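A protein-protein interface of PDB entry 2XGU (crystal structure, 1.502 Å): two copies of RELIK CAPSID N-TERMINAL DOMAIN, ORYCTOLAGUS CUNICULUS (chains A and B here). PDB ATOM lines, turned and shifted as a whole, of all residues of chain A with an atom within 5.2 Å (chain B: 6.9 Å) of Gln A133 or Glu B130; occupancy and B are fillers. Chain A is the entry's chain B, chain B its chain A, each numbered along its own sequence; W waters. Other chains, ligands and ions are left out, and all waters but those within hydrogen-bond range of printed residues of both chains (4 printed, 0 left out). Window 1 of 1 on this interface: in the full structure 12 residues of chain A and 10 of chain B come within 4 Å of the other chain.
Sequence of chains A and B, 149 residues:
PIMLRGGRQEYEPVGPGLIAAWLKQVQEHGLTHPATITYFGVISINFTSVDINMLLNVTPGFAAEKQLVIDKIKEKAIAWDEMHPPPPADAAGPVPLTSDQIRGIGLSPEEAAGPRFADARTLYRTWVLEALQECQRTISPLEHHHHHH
The side-chain carboxylate (OE2) of Glu B130 sits close to the backbone carbonyl oxygen (O) of Glu A130, 3.3 Å away. The side-chain amino group (NZ) of Lys B76 is in salt-bridge range of the side-chain carboxylate (OE2) of Glu A130, 3.5 Å away. OE2 of Glu B130 lies close to OE2 of Glu A134. The side-chain carboxylate (OE2) of Glu B134 lies close to the side-chain carboxylate (OE2) of Glu A130 (3.3 Å). The side-chain amide oxygen (OE1) of Gln A136 is in hydrogen-bond range of the guanidinium group (NH2) of Arg B125 (2.7 Å).
The backbone carbonyl oxygen of Gly B41 lies within hydrogen-bond range of the guanidinium group of Arg B125, 2.8 Å away. The side-chain amino group (NZ) of Lys B76 is in salt-bridge range of the side-chain carboxylate (OE1) of Glu B130. NE2 of Gln A133 lies within hydrogen-bond range of OE1 of Gln A136. The side-chain carboxylate (OE2) of Glu B134 is in salt-bridge range of the side-chain amino group (NZ) of Lys B76 (3.4 Å).
Among the printed residues, pairs that only touch across the chains: Ile A37 with Gln B133 (3.7 Å), Leu A129 with Gln B133 (3.7 Å), Gln A133 with Arg B125 (3.8 Å), Gln A133 with Thr B126 (3.9 Å), Gln A133 with Leu B129 (3.6 Å), Gln A133 with Glu B130 (3.95 Å) and Glu A134 with Thr B126 (3.6 Å).
Of the printed residues of chain B, Ile A37 touches Gln B133 (3.7 Å). Of the printed residues of chain B, Gln A133 touches Arg B125 (3.8 Å), Thr B126 (3.9 Å), Leu B129 (3.6 Å) and Glu B130 (3.95 Å). Ile B37 touches none of the printed residues of chain A. Val B128 touches none of the printed residues of chain A. Of the printed residues of chain A, Leu B129 touches Gln A133 (3.6 Å). Glu B130 touches three residues of chain A. Printed residues of chain A within 4 Å of Gln B133: Ile A37 and Leu A129.
Of the 10 printed residues of chain A, 6 touch a printed residue of chain B. Hydrophobic or aromatic side chains of chain A that line the printed part of chain B: Ile A37 and Leu A129. Among the printed residues, Asp or Glu carboxylates within 4 Å of a Lys or Arg side-chain nitrogen of the other chain: Glu A130 with Lys B76 (3.5 Å).
Ile A37 touches Gln B133, but with the chains exchanged Gln A133 does not touch Ile B37 (6.8 Å). Glu B130 touches its own counterpart, Glu A130. Glu A130 touches Glu B134, and with the chains exchanged Glu A134 touches Glu B130. Gln A133 touches Glu B130, but with the chains exchanged Glu A130 does not touch Gln B133 (6.9 Å).
Water W3 lies within hydrogen-bond range of NZ of Lys B76 (2.5 Å), OE1 of Glu B130 (3.0 Å) and OE2 of Glu A130 (3.4 Å). Water W1 lies within hydrogen-bond range of OE1 of Gln A133 (2.6 Å), NE2 of Gln B133 (2.9 Å) and O of Leu B129 (3.1 Å). Water W2 lies within hydrogen-bond range of the side-chain amide nitrogen of Gln A133 (2.7 Å), the side-chain hydroxyl of Thr B126 (2.9 Å) and the guanidinium group of Arg B125 (3.2 Å). Water W4 bridges OE2 of Glu A134 and OE1 of Glu B130.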
ATOM      1  N   ILE A  37     -17.094  14.896  -1.364  1.00  0.00           N
ATOM      2  CA  ILE A  37     -16.002  14.181  -0.722  1.00  0.00           C
ATOM      3  C   ILE A  37     -16.500  12.816  -0.248  1.00  0.00           C
ATOM      4  O   ILE A  37     -15.864  11.795  -0.464  1.00  0.00           O
ATOM      5  CB  ILE A  37     -15.406  14.997   0.447  1.00  0.00           C
ATOM      6  CG1 ILE A  37     -14.905  16.359  -0.053  1.00  0.00           C
ATOM      7  CG2 ILE A  37     -14.269  14.217   1.140  1.00  0.00           C
ATOM      8  CD1 ILE A  37     -14.161  17.158   1.023  1.00  0.00           C
ATOM      9  N   VAL A 128      -5.803  11.526  -1.224  1.00  0.00           N
ATOM     10  CA  VAL A 128      -6.770  12.250  -2.036  1.00  0.00           C
ATOM     11  C   VAL A 128      -7.936  12.747  -1.186  1.00  0.00           C
ATOM     12  O   VAL A 128      -8.334  13.898  -1.279  1.00  0.00           O
ATOM     13  CB  VAL A 128      -7.272  11.395  -3.216  1.00  0.00           C
ATOM     14  CG1 VAL A 128      -8.367  12.127  -3.960  1.00  0.00           C
ATOM     15  CG2 VAL A 128      -6.113  11.090  -4.155  1.00  0.00           C
ATOM     16  N   LEU A 129      -8.471  11.882  -0.325  1.00  0.00           N
ATOM     17  CA  LEU A 129      -9.520  12.316   0.590  1.00  0.00           C
ATOM     18  C   LEU A 129      -9.065  13.490   1.456  1.00  0.00           C
ATOM     19  O   LEU A 129      -9.830  14.440   1.692  1.00  0.00           O
ATOM     20  CB  LEU A 129      -9.973  11.149   1.482  1.00  0.00           C
ATOM     21  CG  LEU A 129     -10.906  10.132   0.842  1.00  0.00           C
ATOM     22  CD1 LEU A 129     -10.990   8.879   1.719  1.00  0.00           C
ATOM     23  CD2 LEU A 129     -12.298  10.723   0.615  1.00  0.00           C
ATOM     24  N   GLU A 130      -7.843  13.404   1.971  1.00  0.00           N
ATOM     25  CA  GLU A 130      -7.278  14.486   2.777  1.00  0.00           C
ATOM     26  C   GLU A 130      -7.136  15.765   1.947  1.00  0.00           C
ATOM     27  O   GLU A 130      -7.497  16.862   2.404  1.00  0.00           O
ATOM     28  CB  GLU A 130      -5.930  14.064   3.383  1.00  0.00           C
ATOM     29  CG  GLU A 130      -6.075  12.998   4.479  1.00  0.00           C
ATOM     30  CD  GLU A 130      -4.739  12.529   5.019  1.00  0.00           C
ATOM     31  OE1 GLU A 130      -3.698  12.920   4.451  1.00  0.00           O
ATOM     32  OE2 GLU A 130      -4.742  11.767   6.010  1.00  0.00           O
ATOM     33  N   ALA A 131      -6.642  15.633   0.721  1.00  0.00           N
ATOM     34  CA  ALA A 131      -6.466  16.805  -0.129  1.00  0.00           C
ATOM     35  C   ALA A 131      -7.789  17.514  -0.405  1.00  0.00           C
ATOM     36  O   ALA A 131      -7.857  18.738  -0.355  1.00  0.00           O
ATOM     37  CB  ALA A 131      -5.761  16.439  -1.447  1.00  0.00           C
ATOM     38  N   LEU A 132      -8.832  16.749  -0.719  1.00  0.00           N
ATOM     39  CA  LEU A 132     -10.157  17.329  -0.936  1.00  0.00           C
ATOM     40  C   LEU A 132     -10.638  18.085   0.302  1.00  0.00           C
ATOM     41  O   LEU A 132     -11.141  19.202   0.215  1.00  0.00           O
ATOM     42  CB  LEU A 132     -11.161  16.237  -1.288  1.00  0.00           C
ATOM     43  CG  LEU A 132     -10.988  15.545  -2.644  1.00  0.00           C
ATOM     44  CD1 LEU A 132     -11.834  14.270  -2.722  1.00  0.00           C
ATOM     45  CD2 LEU A 132     -11.371  16.515  -3.758  1.00  0.00           C
ATOM     46  N   GLN A 133     -10.486  17.466   1.469  1.00  0.00           N
ATOM     47  CA  GLN A 133     -10.952  18.107   2.705  1.00  0.00           C
ATOM     48  C   GLN A 133     -10.192  19.395   3.002  1.00  0.00           C
ATOM     49  O   GLN A 133     -10.763  20.394   3.447  1.00  0.00           O
ATOM     50  CB  GLN A 133     -10.817  17.147   3.895  1.00  0.00           C
ATOM     51  CG  GLN A 133     -11.514  17.655   5.149  1.00  0.00           C
ATOM     52  CD  GLN A 133     -13.006  17.723   4.940  1.00  0.00           C
ATOM     53  OE1 GLN A 133     -13.624  16.727   4.585  1.00  0.00           O
ATOM     54  NE2 GLN A 133     -13.580  18.902   5.118  1.00  0.00           N
ATOM     55  N   GLU A 134      -8.887  19.354   2.779  1.00  0.00           N
ATOM     56  CA  GLU A 134      -8.028  20.483   3.089  1.00  0.00           C
ATOM     57  C   GLU A 134      -8.279  21.666   2.144  1.00  0.00           C
ATOM     58  O   GLU A 134      -7.935  22.811   2.452  1.00  0.00           O
ATOM     59  CB  GLU A 134      -6.556  20.016   3.124  1.00  0.00           C
ATOM     60  CG  GLU A 134      -6.291  19.115   4.357  1.00  0.00           C
ATOM     61  CD  GLU A 134      -5.100  18.164   4.244  1.00  0.00           C
ATOM     62  OE1 GLU A 134      -4.183  18.419   3.450  1.00  0.00           O
ATOM     63  OE2 GLU A 134      -5.083  17.150   4.977  1.00  0.00           O
ATOM     64  N   CYS A 135      -8.922  21.400   1.014  1.00  0.00           N
ATOM     65  CA  CYS A 135      -9.231  22.443   0.035  1.00  0.00           C
ATOM     66  C   CYS A 135     -10.664  22.927   0.135  1.00  0.00           C
ATOM     67  O   CYS A 135     -11.078  23.815  -0.613  1.00  0.00           O
ATOM     68  CB  CYS A 135      -8.967  21.937  -1.381  1.00  0.00           C
ATOM     69  SG  CYS A 135      -7.223  21.796  -1.733  1.00  0.00           S
ATOM     70  N   GLN A 136     -11.428  22.332   1.042  1.00  0.00           N
ATOM     71  CA  GLN A 136     -12.822  22.706   1.208  1.00  0.00           C
ATOM     72  C   GLN A 136     -12.944  24.115   1.781  1.00  0.00           C
ATOM     73  O   GLN A 136     -12.259  24.466   2.736  1.00  0.00           O
ATOM     74  CB  GLN A 136     -13.513  21.706   2.126  1.00  0.00           C
ATOM     75  CG  GLN A 136     -14.972  22.014   2.379  1.00  0.00           C
ATOM     76  CD  GLN A 136     -15.600  20.952   3.237  1.00  0.00           C
ATOM     77  OE1 GLN A 136     -15.622  21.059   4.468  1.00  0.00           O
ATOM     78  NE2 GLN A 136     -16.074  19.887   2.602  1.00  0.00           N
ATOM     79  N   ILE B  37     -21.536  11.385   7.955  1.00  0.00           N
ATOM     80  CA  ILE B  37     -20.291  12.124   7.757  1.00  0.00           C
ATOM     81  C   ILE B  37     -20.531  13.415   6.958  1.00  0.00           C
ATOM     82  O   ILE B  37     -20.075  14.483   7.335  1.00  0.00           O
ATOM     83  CB  ILE B  37     -19.217  11.248   7.103  1.00  0.00           C
ATOM     84  CG1 ILE B  37     -18.957   9.993   7.954  1.00  0.00           C
ATOM     85  CG2 ILE B  37     -17.946  12.067   6.889  1.00  0.00           C
ATOM     86  CD1 ILE B  37     -18.056   8.935   7.270  1.00  0.00           C
ATOM     87  N   GLY B  41     -20.119  17.314   8.272  1.00  0.00           N
ATOM     88  CA  GLY B  41     -19.426  18.321   7.484  1.00  0.00           C
ATOM     89  C   GLY B  41     -20.239  19.605   7.330  1.00  0.00           C
ATOM     90  O   GLY B  41     -19.717  20.699   7.484  1.00  0.00           O
ATOM     91  N   LYS B  72      -7.785   7.786  14.962  1.00  0.00           N
ATOM     92  CA  LYS B  72      -7.223   8.427  13.781  1.00  0.00           C
ATOM     93  C   LYS B  72      -6.897   9.895  14.049  1.00  0.00           C
ATOM     94  O   LYS B  72      -5.883  10.391  13.579  1.00  0.00           O
ATOM     95  CB  LYS B  72      -8.124   8.257  12.554  1.00  0.00           C
ATOM     96  CG  LYS B  72      -8.108   6.839  12.020  1.00  0.00           C
ATOM     97  CD  LYS B  72      -8.889   6.699  10.735  1.00  0.00           C
ATOM     98  CE  LYS B  72      -8.832   5.255  10.250  1.00  0.00           C
ATOM     99  NZ  LYS B  72      -7.439   4.729  10.224  1.00  0.00           N
ATOM    100  N   LYS B  76      -3.133  11.728  13.825  1.00  0.00           N
ATOM    101  CA  LYS B  76      -2.859  13.011  13.178  1.00  0.00           C
ATOM    102  C   LYS B  76      -2.163  13.981  14.125  1.00  0.00           C
ATOM    103  O   LYS B  76      -1.266  14.727  13.721  1.00  0.00           O
ATOM    104  CB  LYS B  76      -4.150  13.661  12.682  1.00  0.00           C
ATOM    105  CG  LYS B  76      -4.877  12.874  11.603  1.00  0.00           C
ATOM    106  CD  LYS B  76      -6.146  13.613  11.183  1.00  0.00           C
ATOM    107  CE  LYS B  76      -7.033  12.765  10.297  1.00  0.00           C
ATOM    108  NZ  LYS B  76      -6.303  12.277   9.089  1.00  0.00           N
ATOM    109  N   LEU B 123      -8.517  23.750  11.040  1.00  0.00           N
ATOM    110  CA  LEU B 123      -7.638  22.592  10.902  1.00  0.00           C
ATOM    111  C   LEU B 123      -8.169  21.397  11.697  1.00  0.00           C
ATOM    112  O   LEU B 123      -8.121  20.249  11.225  1.00  0.00           O
ATOM    113  CB  LEU B 123      -6.221  22.953  11.350  1.00  0.00           C
ATOM    114  CG  LEU B 123      -5.210  21.816  11.248  1.00  0.00           C
ATOM    115  CD1 LEU B 123      -5.055  21.343   9.810  1.00  0.00           C
ATOM    116  CD2 LEU B 123      -3.853  22.247  11.817  1.00  0.00           C
ATOM    117  N   TYR B 124      -8.688  21.653  12.891  1.00  0.00           N
ATOM    118  CA  TYR B 124      -9.219  20.553  13.696  1.00  0.00           C
ATOM    119  C   TYR B 124     -10.441  19.921  13.028  1.00  0.00           C
ATOM    120  O   TYR B 124     -10.589  18.692  13.022  1.00  0.00           O
ATOM    121  CB  TYR B 124      -9.584  21.018  15.110  1.00  0.00           C
ATOM    122  CG  TYR B 124     -10.037  19.909  16.038  1.00  0.00           C
ATOM    123  CD1 TYR B 124      -9.343  18.708  16.107  1.00  0.00           C
ATOM    124  CD2 TYR B 124     -11.153  20.072  16.847  1.00  0.00           C
ATOM    125  CE1 TYR B 124      -9.730  17.693  16.965  1.00  0.00           C
ATOM    126  CE2 TYR B 124     -11.552  19.065  17.718  1.00  0.00           C
ATOM    127  CZ  TYR B 124     -10.845  17.876  17.763  1.00  0.00           C
ATOM    128  OH  TYR B 124     -11.225  16.867  18.625  1.00  0.00           O
ATOM    129  N   ARG B 125     -11.326  20.759  12.496  1.00  0.00           N
ATOM    130  CA  ARG B 125     -12.476  20.261  11.753  1.00  0.00           C
ATOM    131  C   ARG B 125     -12.014  19.376  10.597  1.00  0.00           C
ATOM    132  O   ARG B 125     -12.590  18.311  10.364  1.00  0.00           O
ATOM    133  CB  ARG B 125     -13.339  21.417  11.245  1.00  0.00           C
ATOM    134  CG  ARG B 125     -14.465  20.988  10.310  1.00  0.00           C
ATOM    135  CD  ARG B 125     -15.298  22.193   9.873  1.00  0.00           C
ATOM    136  NE  ARG B 125     -16.312  21.798   8.895  1.00  0.00           N
ATOM    137  CZ  ARG B 125     -16.085  21.669   7.592  1.00  0.00           C
ATOM    138  NH1 ARG B 125     -14.881  21.933   7.088  1.00  0.00           N
ATOM    139  NH2 ARG B 125     -17.066  21.271   6.783  1.00  0.00           N
ATOM    140  N   THR B 126     -10.974  19.812   9.889  1.00  0.00           N
ATOM    141  CA  THR B 126     -10.373  19.005   8.838  1.00  0.00           C
ATOM    142  C   THR B 126      -9.891  17.646   9.349  1.00  0.00           C
ATOM    143  O   THR B 126     -10.198  16.616   8.755  1.00  0.00           O
ATOM    144  CB  THR B 126      -9.230  19.778   8.164  1.00  0.00           C
ATOM    145  OG1 THR B 126      -9.792  20.860   7.415  1.00  0.00           O
ATOM    146  CG2 THR B 126      -8.425  18.872   7.240  1.00  0.00           C
ATOM    147  N   TRP B 127      -9.171  17.627  10.472  1.00  0.00           N
ATOM    148  CA  TRP B 127      -8.726  16.363  11.065  1.00  0.00           C
ATOM    149  C   TRP B 127      -9.899  15.433  11.400  1.00  0.00           C
ATOM    150  O   TRP B 127      -9.850  14.236  11.112  1.00  0.00           O
ATOM    151  CB  TRP B 127      -7.940  16.614  12.364  1.00  0.00           C
ATOM    152  CG  TRP B 127      -6.574  17.212  12.168  1.00  0.00           C
ATOM    153  CD1 TRP B 127      -5.974  17.525  10.992  1.00  0.00           C
ATOM    154  CD2 TRP B 127      -5.645  17.576  13.203  1.00  0.00           C
ATOM    155  NE1 TRP B 127      -4.716  18.056  11.220  1.00  0.00           N
ATOM    156  CE2 TRP B 127      -4.500  18.103  12.572  1.00  0.00           C
ATOM    157  CE3 TRP B 127      -5.677  17.509  14.598  1.00  0.00           C
ATOM    158  CZ2 TRP B 127      -3.396  18.556  13.292  1.00  0.00           C
ATOM    159  CZ3 TRP B 127      -4.579  17.958  15.315  1.00  0.00           C
ATOM    160  CH2 TRP B 127      -3.452  18.464  14.658  1.00  0.00           C
ATOM    161  N   VAL B 128     -10.946  15.980  12.009  1.00  0.00           N
ATOM    162  CA  VAL B 128     -12.087  15.163  12.415  1.00  0.00           C
ATOM    163  C   VAL B 128     -12.817  14.593  11.197  1.00  0.00           C
ATOM    164  O   VAL B 128     -13.154  13.405  11.155  1.00  0.00           O
ATOM    165  CB  VAL B 128     -13.045  15.979  13.309  1.00  0.00           C
ATOM    166  CG1 VAL B 128     -14.291  15.176  13.656  1.00  0.00           C
ATOM    167  CG2 VAL B 128     -12.329  16.393  14.589  1.00  0.00           C
ATOM    168  N   LEU B 129     -13.047  15.434  10.192  1.00  0.00           N
ATOM    169  CA  LEU B 129     -13.696  14.955   8.982  1.00  0.00           C
ATOM    170  C   LEU B 129     -12.825  13.932   8.242  1.00  0.00           C
ATOM    171  O   LEU B 129     -13.340  12.928   7.740  1.00  0.00           O
ATOM    172  CB  LEU B 129     -14.136  16.136   8.090  1.00  0.00           C
ATOM    173  CG  LEU B 129     -15.421  16.810   8.619  1.00  0.00           C
ATOM    174  CD1 LEU B 129     -15.638  18.218   8.081  1.00  0.00           C
ATOM    175  CD2 LEU B 129     -16.652  15.932   8.319  1.00  0.00           C
ATOM    176  N   GLU B 130     -11.515  14.153   8.190  1.00  0.00           N
ATOM    177  CA  GLU B 130     -10.634  13.154   7.594  1.00  0.00           C
ATOM    178  C   GLU B 130     -10.739  11.827   8.345  1.00  0.00           C
ATOM    179  O   GLU B 130     -10.807  10.770   7.733  1.00  0.00           O
ATOM    180  CB  GLU B 130      -9.190  13.651   7.555  1.00  0.00           C
ATOM    181  CG  GLU B 130      -9.047  14.803   6.568  1.00  0.00           C
ATOM    182  CD  GLU B 130      -7.679  15.425   6.570  1.00  0.00           C
ATOM    183  OE1 GLU B 130      -6.887  15.109   7.478  1.00  0.00           O
ATOM    184  OE2 GLU B 130      -7.396  16.223   5.649  1.00  0.00           O
ATOM    185  N   ALA B 131     -10.764  11.881   9.673  1.00  0.00           N
ATOM    186  CA  ALA B 131     -10.849  10.669  10.475  1.00  0.00           C
ATOM    187  C   ALA B 131     -12.153   9.920  10.225  1.00  0.00           C
ATOM    188  O   ALA B 131     -12.156   8.704  10.040  1.00  0.00           O
ATOM    189  CB  ALA B 131     -10.691  10.999  11.954  1.00  0.00           C
ATOM    190  N   LEU B 132     -13.260  10.653  10.217  1.00  0.00           N
ATOM    191  CA  LEU B 132     -14.555  10.047   9.892  1.00  0.00           C
ATOM    192  C   LEU B 132     -14.548   9.401   8.505  1.00  0.00           C
ATOM    193  O   LEU B 132     -14.977   8.257   8.326  1.00  0.00           O
ATOM    194  CB  LEU B 132     -15.677  11.080   9.993  1.00  0.00           C
ATOM    195  CG  LEU B 132     -16.010  11.544  11.402  1.00  0.00           C
ATOM    196  CD1 LEU B 132     -16.810  12.834  11.370  1.00  0.00           C
ATOM    197  CD2 LEU B 132     -16.802  10.434  12.084  1.00  0.00           C
ATOM    198  N   GLN B 133     -14.064  10.147   7.517  1.00  0.00           N
ATOM    199  CA  GLN B 133     -14.027   9.668   6.144  1.00  0.00           C
ATOM    200  C   GLN B 133     -13.226   8.375   6.023  1.00  0.00           C
ATOM    201  O   GLN B 133     -13.607   7.463   5.277  1.00  0.00           O
ATOM    202  CB  GLN B 133     -13.402  10.750   5.265  1.00  0.00           C
ATOM    203  CG  GLN B 133     -14.042  11.010   3.903  1.00  0.00           C
ATOM    204  CD  GLN B 133     -15.504  11.434   3.964  1.00  0.00           C
ATOM    205  OE1 GLN B 133     -16.385  10.610   3.782  1.00  0.00           O
ATOM    206  NE2 GLN B 133     -15.762  12.721   4.189  1.00  0.00           N
ATOM    207  N   GLU B 134     -12.119   8.289   6.758  1.00  0.00           N
ATOM    208  CA  GLU B 134     -11.246   7.118   6.715  1.00  0.00           C
ATOM    209  C   GLU B 134     -11.848   5.902   7.437  1.00  0.00           C
ATOM    210  O   GLU B 134     -11.358   4.783   7.288  1.00  0.00           O
ATOM    211  CB  GLU B 134      -9.843   7.470   7.242  1.00  0.00           C
ATOM    212  CG  GLU B 134      -9.126   8.496   6.348  1.00  0.00           C
ATOM    213  CD  GLU B 134      -8.018   9.292   7.047  1.00  0.00           C
ATOM    214  OE1 GLU B 134      -7.496   8.827   8.086  1.00  0.00           O
ATOM    215  OE2 GLU B 134      -7.667  10.391   6.547  1.00  0.00           O
ATOM    216  N   CYS B 135     -12.925   6.121   8.189  1.00  0.00           N
ATOM    217  CA  CYS B 135     -13.627   5.039   8.881  1.00  0.00           C
ATOM    218  C   CYS B 135     -15.001   4.794   8.267  1.00  0.00           C
ATOM    219  O   CYS B 135     -15.850   4.141   8.864  1.00  0.00           O
ATOM    220  CB  CYS B 135     -13.800   5.373  10.365  1.00  0.00           C
ATOM    221  SG  CYS B 135     -12.275   5.559  11.282  1.00  0.00           S
HETATM  222  O   HOH W   1     -13.413  14.184   4.919  1.00  0.00           O
HETATM  223  O   HOH W   2     -12.135  21.097   5.702  1.00  0.00           O
HETATM  224  O   HOH W   3      -4.389  13.881   8.588  1.00  0.00           O
HETATM  225  O   HOH W   4      -3.791  16.096   7.554  1.00  0.00           O
